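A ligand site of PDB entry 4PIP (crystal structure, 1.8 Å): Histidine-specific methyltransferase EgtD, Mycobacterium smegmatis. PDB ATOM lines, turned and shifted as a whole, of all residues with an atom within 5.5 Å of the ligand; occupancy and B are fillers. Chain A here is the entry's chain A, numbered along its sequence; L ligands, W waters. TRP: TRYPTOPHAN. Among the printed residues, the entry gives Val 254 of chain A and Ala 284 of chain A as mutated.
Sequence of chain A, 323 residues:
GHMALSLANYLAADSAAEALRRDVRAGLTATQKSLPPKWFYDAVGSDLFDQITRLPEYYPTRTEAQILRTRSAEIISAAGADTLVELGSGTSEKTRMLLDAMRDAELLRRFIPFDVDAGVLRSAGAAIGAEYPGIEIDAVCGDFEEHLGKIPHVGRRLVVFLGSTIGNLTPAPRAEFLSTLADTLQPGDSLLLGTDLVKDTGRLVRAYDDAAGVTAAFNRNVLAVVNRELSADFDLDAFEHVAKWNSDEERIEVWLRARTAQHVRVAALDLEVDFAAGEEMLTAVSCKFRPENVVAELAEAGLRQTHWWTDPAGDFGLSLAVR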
ATOM      1  N   PRO A  37      12.486 -19.425  15.415  1.00  0.00           N
ATOM      2  CA  PRO A  37      12.847 -18.054  15.776  1.00  0.00           C
ATOM      3  C   PRO A  37      12.211 -17.541  17.072  1.00  0.00           C
ATOM      4  O   PRO A  37      12.658 -16.501  17.549  1.00  0.00           O
ATOM      5  CB  PRO A  37      12.338 -17.224  14.581  1.00  0.00           C
ATOM      6  CG  PRO A  37      11.366 -18.071  13.899  1.00  0.00           C
ATOM      7  CD  PRO A  37      11.785 -19.477  14.121  1.00  0.00           C
ATOM      8  N   PHE A  40      14.669 -16.618  19.931  1.00  0.00           N
ATOM      9  CA  PHE A  40      15.695 -15.579  19.806  1.00  0.00           C
ATOM     10  C   PHE A  40      15.619 -14.578  20.960  1.00  0.00           C
ATOM     11  O   PHE A  40      16.629 -13.996  21.313  1.00  0.00           O
ATOM     12  CB  PHE A  40      15.571 -14.819  18.478  1.00  0.00           C
ATOM     13  CG  PHE A  40      16.195 -15.506  17.307  1.00  0.00           C
ATOM     14  CD1 PHE A  40      16.003 -16.855  17.089  1.00  0.00           C
ATOM     15  CD2 PHE A  40      16.946 -14.795  16.386  1.00  0.00           C
ATOM     16  CE1 PHE A  40      16.579 -17.497  16.002  1.00  0.00           C
ATOM     17  CE2 PHE A  40      17.511 -15.412  15.285  1.00  0.00           C
ATOM     18  CZ  PHE A  40      17.328 -16.757  15.089  1.00  0.00           C
ATOM     19  N   TYR A  41      14.449 -14.377  21.563  1.00  0.00           N
ATOM     20  CA  TYR A  41      14.223 -13.155  22.324  1.00  0.00           C
ATOM     21  C   TYR A  41      14.332 -13.276  23.853  1.00  0.00           C
ATOM     22  O   TYR A  41      13.470 -12.764  24.569  1.00  0.00           O
ATOM     23  CB  TYR A  41      12.848 -12.581  21.970  1.00  0.00           C
ATOM     24  CG  TYR A  41      12.627 -12.467  20.473  1.00  0.00           C
ATOM     25  CD1 TYR A  41      12.194 -13.560  19.720  1.00  0.00           C
ATOM     26  CD2 TYR A  41      12.874 -11.272  19.812  1.00  0.00           C
ATOM     27  CE1 TYR A  41      11.993 -13.425  18.336  1.00  0.00           C
ATOM     28  CE2 TYR A  41      12.691 -11.145  18.458  1.00  0.00           C
ATOM     29  CZ  TYR A  41      12.255 -12.212  17.723  1.00  0.00           C
ATOM     30  OH  TYR A  41      12.070 -12.019  16.357  1.00  0.00           O
ATOM     31  N   PHE A  49      17.478  -7.092  19.444  1.00  0.00           N
ATOM     32  CA  PHE A  49      16.336  -6.761  18.551  1.00  0.00           C
ATOM     33  C   PHE A  49      16.049  -5.275  18.654  1.00  0.00           C
ATOM     34  O   PHE A  49      15.952  -4.631  17.691  1.00  0.00           O
ATOM     35  CB  PHE A  49      15.070  -7.486  18.870  1.00  0.00           C
ATOM     36  CG  PHE A  49      13.978  -7.187  17.887  1.00  0.00           C
ATOM     37  CD1 PHE A  49      14.004  -7.733  16.699  1.00  0.00           C
ATOM     38  CD2 PHE A  49      13.022  -6.311  18.163  1.00  0.00           C
ATOM     39  CE1 PHE A  49      13.040  -7.456  15.749  1.00  0.00           C
ATOM     40  CE2 PHE A  49      12.035  -6.002  17.241  1.00  0.00           C
ATOM     41  CZ  PHE A  49      12.065  -6.580  16.023  1.00  0.00           C
ATOM     42  N   ILE A  52      18.408  -3.648  16.499  1.00  0.00           N
ATOM     43  CA  ILE A  52      17.971  -3.859  15.132  1.00  0.00           C
ATOM     44  C   ILE A  52      16.924  -2.825  14.676  1.00  0.00           C
ATOM     45  O   ILE A  52      17.007  -2.311  13.559  1.00  0.00           O
ATOM     46  CB  ILE A  52      17.409  -5.287  14.950  1.00  0.00           C
ATOM     47  CG1 ILE A  52      18.561  -6.284  15.058  1.00  0.00           C
ATOM     48  CG2 ILE A  52      16.718  -5.420  13.580  1.00  0.00           C
ATOM     49  CD1 ILE A  52      18.157  -7.750  14.938  1.00  0.00           C
ATOM     50  N   TYR A  58      17.263  -1.618   8.522  1.00  0.00           N
ATOM     51  CA  TYR A  58      16.039  -2.247   9.019  1.00  0.00           C
ATOM     52  C   TYR A  58      14.927  -1.209   9.135  1.00  0.00           C
ATOM     53  O   TYR A  58      14.680  -0.661  10.194  1.00  0.00           O
ATOM     54  CB  TYR A  58      16.267  -2.926  10.378  1.00  0.00           C
ATOM     55  CG  TYR A  58      15.106  -3.823  10.736  1.00  0.00           C
ATOM     56  CD1 TYR A  58      14.979  -5.077  10.142  1.00  0.00           C
ATOM     57  CD2 TYR A  58      14.125  -3.424  11.631  1.00  0.00           C
ATOM     58  CE1 TYR A  58      13.920  -5.896  10.436  1.00  0.00           C
ATOM     59  CE2 TYR A  58      13.064  -4.236  11.937  1.00  0.00           C
ATOM     60  CZ  TYR A  58      12.967  -5.476  11.339  1.00  0.00           C
ATOM     61  OH  TYR A  58      11.890  -6.300  11.609  1.00  0.00           O
ATOM     62  N   PRO A  60      11.558  -1.771   8.764  1.00  0.00           N
ATOM     63  CA  PRO A  60      10.203  -2.118   9.233  1.00  0.00           C
ATOM     64  C   PRO A  60       9.681  -1.433  10.504  1.00  0.00           C
ATOM     65  O   PRO A  60       8.518  -1.059  10.522  1.00  0.00           O
ATOM     66  CB  PRO A  60      10.295  -3.623   9.467  1.00  0.00           C
ATOM     67  CG  PRO A  60      11.295  -4.078   8.483  1.00  0.00           C
ATOM     68  CD  PRO A  60      12.323  -2.987   8.426  1.00  0.00           C
ATOM     69  N   GLY A 163       4.920  -5.715  13.761  1.00  0.00           N
ATOM     70  CA  GLY A 163       6.329  -5.986  13.486  1.00  0.00           C
ATOM     71  C   GLY A 163       6.561  -7.004  12.389  1.00  0.00           C
ATOM     72  O   GLY A 163       7.696  -7.447  12.140  1.00  0.00           O
ATOM     73  N   SER A 164       5.487  -7.378  11.707  1.00  0.00           N
ATOM     74  CA  SER A 164       5.523  -8.449  10.708  1.00  0.00           C
ATOM     75  C   SER A 164       5.969  -9.771  11.323  1.00  0.00           C
ATOM     76  O   SER A 164       6.523 -10.628  10.640  1.00  0.00           O
ATOM     77  CB  SER A 164       6.438  -8.074   9.550  1.00  0.00           C
ATOM     78  OG  SER A 164       6.038  -8.771   8.384  1.00  0.00           O
ATOM     79  N   THR A 165       5.686  -9.932  12.616  1.00  0.00           N
ATOM     80  CA  THR A 165       5.969 -11.169  13.329  1.00  0.00           C
ATOM     81  C   THR A 165       5.189 -12.318  12.684  1.00  0.00           C
ATOM     82  O   THR A 165       5.665 -13.457  12.655  1.00  0.00           O
ATOM     83  CB  THR A 165       5.615 -11.048  14.850  1.00  0.00           C
ATOM     84  OG1 THR A 165       6.353  -9.982  15.447  1.00  0.00           O
ATOM     85  CG2 THR A 165       5.929 -12.333  15.593  1.00  0.00           C
ATOM     86  N   ASN A 168       7.046 -14.445  10.311  1.00  0.00           N
ATOM     87  CA  ASN A 168       8.023 -15.382  10.845  1.00  0.00           C
ATOM     88  C   ASN A 168       7.389 -16.775  10.920  1.00  0.00           C
ATOM     89  O   ASN A 168       8.006 -17.707  11.422  1.00  0.00           O
ATOM     90  CB  ASN A 168       8.548 -14.914  12.211  1.00  0.00           C
ATOM     91  CG  ASN A 168       9.253 -13.551  12.152  1.00  0.00           C
ATOM     92  OD1 ASN A 168       8.988 -12.686  12.981  1.00  0.00           O
ATOM     93  ND2 ASN A 168      10.154 -13.374  11.164  1.00  0.00           N
ATOM     94  N   ALA A 207      18.318  -5.500   5.111  1.00  0.00           N
ATOM     95  CA  ALA A 207      17.564  -5.340   6.335  1.00  0.00           C
ATOM     96  C   ALA A 207      17.850  -6.462   7.334  1.00  0.00           C
ATOM     97  O   ALA A 207      17.649  -6.300   8.542  1.00  0.00           O
ATOM     98  CB  ALA A 207      16.080  -5.270   6.001  1.00  0.00           C
ATOM     99  N   TYR A 208      18.343  -7.598   6.836  1.00  0.00           N
ATOM    100  CA  TYR A 208      18.661  -8.749   7.693  1.00  0.00           C
ATOM    101  C   TYR A 208      20.158  -9.097   7.631  1.00  0.00           C
ATOM    102  O   TYR A 208      20.560 -10.217   7.906  1.00  0.00           O
ATOM    103  CB  TYR A 208      17.806  -9.947   7.269  1.00  0.00           C
ATOM    104  CG  TYR A 208      16.362  -9.603   7.427  1.00  0.00           C
ATOM    105  CD1 TYR A 208      15.706  -9.794   8.625  1.00  0.00           C
ATOM    106  CD2 TYR A 208      15.643  -9.014   6.366  1.00  0.00           C
ATOM    107  CE1 TYR A 208      14.372  -9.441   8.783  1.00  0.00           C
ATOM    108  CE2 TYR A 208      14.319  -8.662   6.524  1.00  0.00           C
ATOM    109  CZ  TYR A 208      13.694  -8.864   7.732  1.00  0.00           C
ATOM    110  OH  TYR A 208      12.379  -8.504   7.903  1.00  0.00           O
ATOM    111  N   THR A 215      22.541  -7.791  13.309  1.00  0.00           N
ATOM    112  CA  THR A 215      21.652  -8.888  12.997  1.00  0.00           C
ATOM    113  C   THR A 215      22.406 -10.203  13.131  1.00  0.00           C
ATOM    114  O   THR A 215      21.840 -11.218  13.533  1.00  0.00           O
ATOM    115  CB  THR A 215      21.043  -8.785  11.588  1.00  0.00           C
ATOM    116  OG1 THR A 215      20.313  -7.555  11.461  1.00  0.00           O
ATOM    117  CG2 THR A 215      20.085  -9.964  11.320  1.00  0.00           C
ATOM    118  N   PHE A 218      22.499 -11.106  16.767  1.00  0.00           N
ATOM    119  CA  PHE A 218      21.136 -11.521  17.111  1.00  0.00           C
ATOM    120  C   PHE A 218      20.914 -12.985  16.709  1.00  0.00           C
ATOM    121  O   PHE A 218      20.469 -13.805  17.502  1.00  0.00           O
ATOM    122  CB  PHE A 218      20.140 -10.586  16.439  1.00  0.00           C
ATOM    123  CG  PHE A 218      18.682 -10.912  16.668  1.00  0.00           C
ATOM    124  CD1 PHE A 218      18.129 -10.845  17.940  1.00  0.00           C
ATOM    125  CD2 PHE A 218      17.867 -11.271  15.609  1.00  0.00           C
ATOM    126  CE1 PHE A 218      16.792 -11.144  18.142  1.00  0.00           C
ATOM    127  CE2 PHE A 218      16.529 -11.548  15.807  1.00  0.00           C
ATOM    128  CZ  PHE A 218      15.986 -11.491  17.077  1.00  0.00           C
ATOM    129  N   VAL A 254      16.947 -16.822   6.918  1.00  0.00           N
ATOM    130  CA  VAL A 254      18.115 -16.549   7.753  1.00  0.00           C
ATOM    131  C   VAL A 254      18.730 -17.852   8.238  1.00  0.00           C
ATOM    132  O   VAL A 254      18.033 -18.693   8.799  1.00  0.00           O
ATOM    133  CB  VAL A 254      17.730 -15.692   8.970  1.00  0.00           C
ATOM    134  CG1 VAL A 254      18.886 -15.546   9.913  1.00  0.00           C
ATOM    135  CG2 VAL A 254      17.270 -14.324   8.515  1.00  0.00           C
ATOM    136  N   ALA A 284      15.473 -18.678  10.870  1.00  0.00           N
ATOM    137  CA  ALA A 284      14.255 -17.883  10.687  1.00  0.00           C
ATOM    138  C   ALA A 284      13.858 -17.721   9.235  1.00  0.00           C
ATOM    139  O   ALA A 284      14.702 -17.774   8.342  1.00  0.00           O
ATOM    140  CB  ALA A 284      14.414 -16.487  11.304  1.00  0.00           C
ATOM    141  N   VAL A 285      12.560 -17.491   9.003  1.00  0.00           N
ATOM    142  CA  VAL A 285      12.098 -16.923   7.753  1.00  0.00           C
ATOM    143  C   VAL A 285      11.427 -15.611   8.104  1.00  0.00           C
ATOM    144  O   VAL A 285      10.989 -15.401   9.238  1.00  0.00           O
ATOM    145  CB  VAL A 285      11.126 -17.835   6.968  1.00  0.00           C
ATOM    146  CG1 VAL A 285      11.749 -19.212   6.751  1.00  0.00           C
ATOM    147  CG2 VAL A 285       9.773 -17.968   7.668  1.00  0.00           C
ATOM    148  N   SER A 286      11.392 -14.727   7.123  1.00  0.00           N
ATOM    149  CA  SER A 286      10.613 -13.497   7.234  1.00  0.00           C
ATOM    150  C   SER A 286       9.873 -13.304   5.916  1.00  0.00           C
ATOM    151  O   SER A 286      10.404 -12.763   4.951  1.00  0.00           O
ATOM    152  CB  SER A 286      11.508 -12.304   7.544  1.00  0.00           C
ATOM    153  OG  SER A 286      10.703 -11.189   7.932  1.00  0.00           O
ATOM    154  N   LYS A 288       7.454 -11.884   3.094  1.00  0.00           N
ATOM    155  CA  LYS A 288       7.037 -10.562   2.627  1.00  0.00           C
ATOM    156  C   LYS A 288       5.774 -10.700   1.774  1.00  0.00           C
ATOM    157  O   LYS A 288       5.649 -11.617   0.957  1.00  0.00           O
ATOM    158  CB  LYS A 288       8.161  -9.897   1.842  1.00  0.00           C
ATOM    159  CG  LYS A 288       9.475  -9.858   2.616  1.00  0.00           C
ATOM    160  CD  LYS A 288       9.308  -9.154   3.978  1.00  0.00           C
ATOM    161  CE  LYS A 288      10.602  -9.165   4.778  1.00  0.00           C
ATOM    162  NZ  LYS A 288      10.382  -8.604   6.115  1.00  0.00           N
HETATM  163  N   TRP L   1       9.587  -9.766  12.965  1.00  0.00           N
HETATM  164  CA  TRP L   1      10.985  -9.413  12.594  1.00  0.00           C
HETATM  165  C   TRP L   1      11.136  -9.533  11.093  1.00  0.00           C
HETATM  166  O   TRP L   1      11.451  -8.537  10.449  1.00  0.00           O
HETATM  167  CB  TRP L   1      11.985 -10.320  13.316  1.00  0.00           C
HETATM  168  CG  TRP L   1      13.409 -10.169  12.855  1.00  0.00           C
HETATM  169  CD1 TRP L   1      14.061  -9.001  12.557  1.00  0.00           C
HETATM  170  CD2 TRP L   1      14.357 -11.215  12.653  1.00  0.00           C
HETATM  171  NE1 TRP L   1      15.367  -9.273  12.191  1.00  0.00           N
HETATM  172  CE2 TRP L   1      15.566 -10.621  12.238  1.00  0.00           C
HETATM  173  CE3 TRP L   1      14.300 -12.609  12.796  1.00  0.00           C
HETATM  174  CZ2 TRP L   1      16.699 -11.374  11.938  1.00  0.00           C
HETATM  175  CZ3 TRP L   1      15.411 -13.346  12.509  1.00  0.00           C
HETATM  176  CH2 TRP L   1      16.601 -12.738  12.076  1.00  0.00           C
HETATM  177  OXT TRP L   1      10.920 -10.595  10.499  1.00  0.00           O
HETATM  178  O   HOH W   1       9.243  -9.913  15.430  1.00  0.00           O
HETATM  179  O   HOH W   2      17.538  -7.675  10.936  1.00  0.00           O
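The side-chain amide nitrogen of Asn 168 lies within hydrogen-bond range of an oxygen (OXT) of the ligand (3.0 Å).
A nitrogen (N) of the ligand sits at hydrogen-bond distance from the backbone carbonyl oxygen (O) of Gly 163 (3.1 Å).
OXT of the ligand is in hydrogen-bond range of OG of Ser 286 (2.6 Å).
The side-chain hydroxyl of Tyr 208 is in hydrogen-bond range of an oxygen (O) of the ligand (2.7 Å).
OH of Tyr 58 sits at hydrogen-bond distance from O of the ligand, at 2.6 Å.
Residues that only touch the ligand: Tyr 41 (3.5 Å), Ala 284 (3.5 Å), Phe 49 (3.7 Å), Thr 215 (3.7 Å), Phe 218 (3.8 Å), Thr 165 (3.9 Å), Ser 164 (3.9 Å) and Val 254 (3.96 Å).
Hydrophobic or aromatic side chains within 4 Å of the ligand: Phe 49, Tyr 58, Tyr 208, Phe 218, Val 254 and Ala 284.
Water W1 lies within hydrogen-bond range of N of the ligand (2.5 Å) and OG1 of Thr 165 (2.9 Å).
Water W2 lies within hydrogen-bond range of the backbone carbonyl oxygen (O) of Ala 207 (2.8 Å), the side-chain hydroxyl (OG1) of Thr 215 (2.8 Å) and a nitrogen (NE1) of the ligand (3.0 Å).
The side-chain amide oxygen (OD1) of Asn 168 sits close to the backbone carbonyl oxygen (O) of Thr 165 (3.4 Å).
The side-chain hydroxyl (OH) of Tyr 208 lies within hydrogen-bond range of the side-chain hydroxyl (OG) of Ser 286 (3.2 Å).
O of Ala 284 lies within hydrogen-bond range of N of Val 254, 2.8 Å away.
The side-chain amino group (NZ) of Lys 288 sits at hydrogen-bond distance from the side-chain hydroxyl (OH) of Tyr 208.
The side-chain amide nitrogen (ND2) of Asn 168 sits at hydrogen-bond distance from the backbone carbonyl oxygen (O) of Val 285 (2.9 Å).
The side-chain amino group (NZ) of Lys 288 lies within hydrogen-bond range of the side-chain hydroxyl (OG) of Ser 286.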
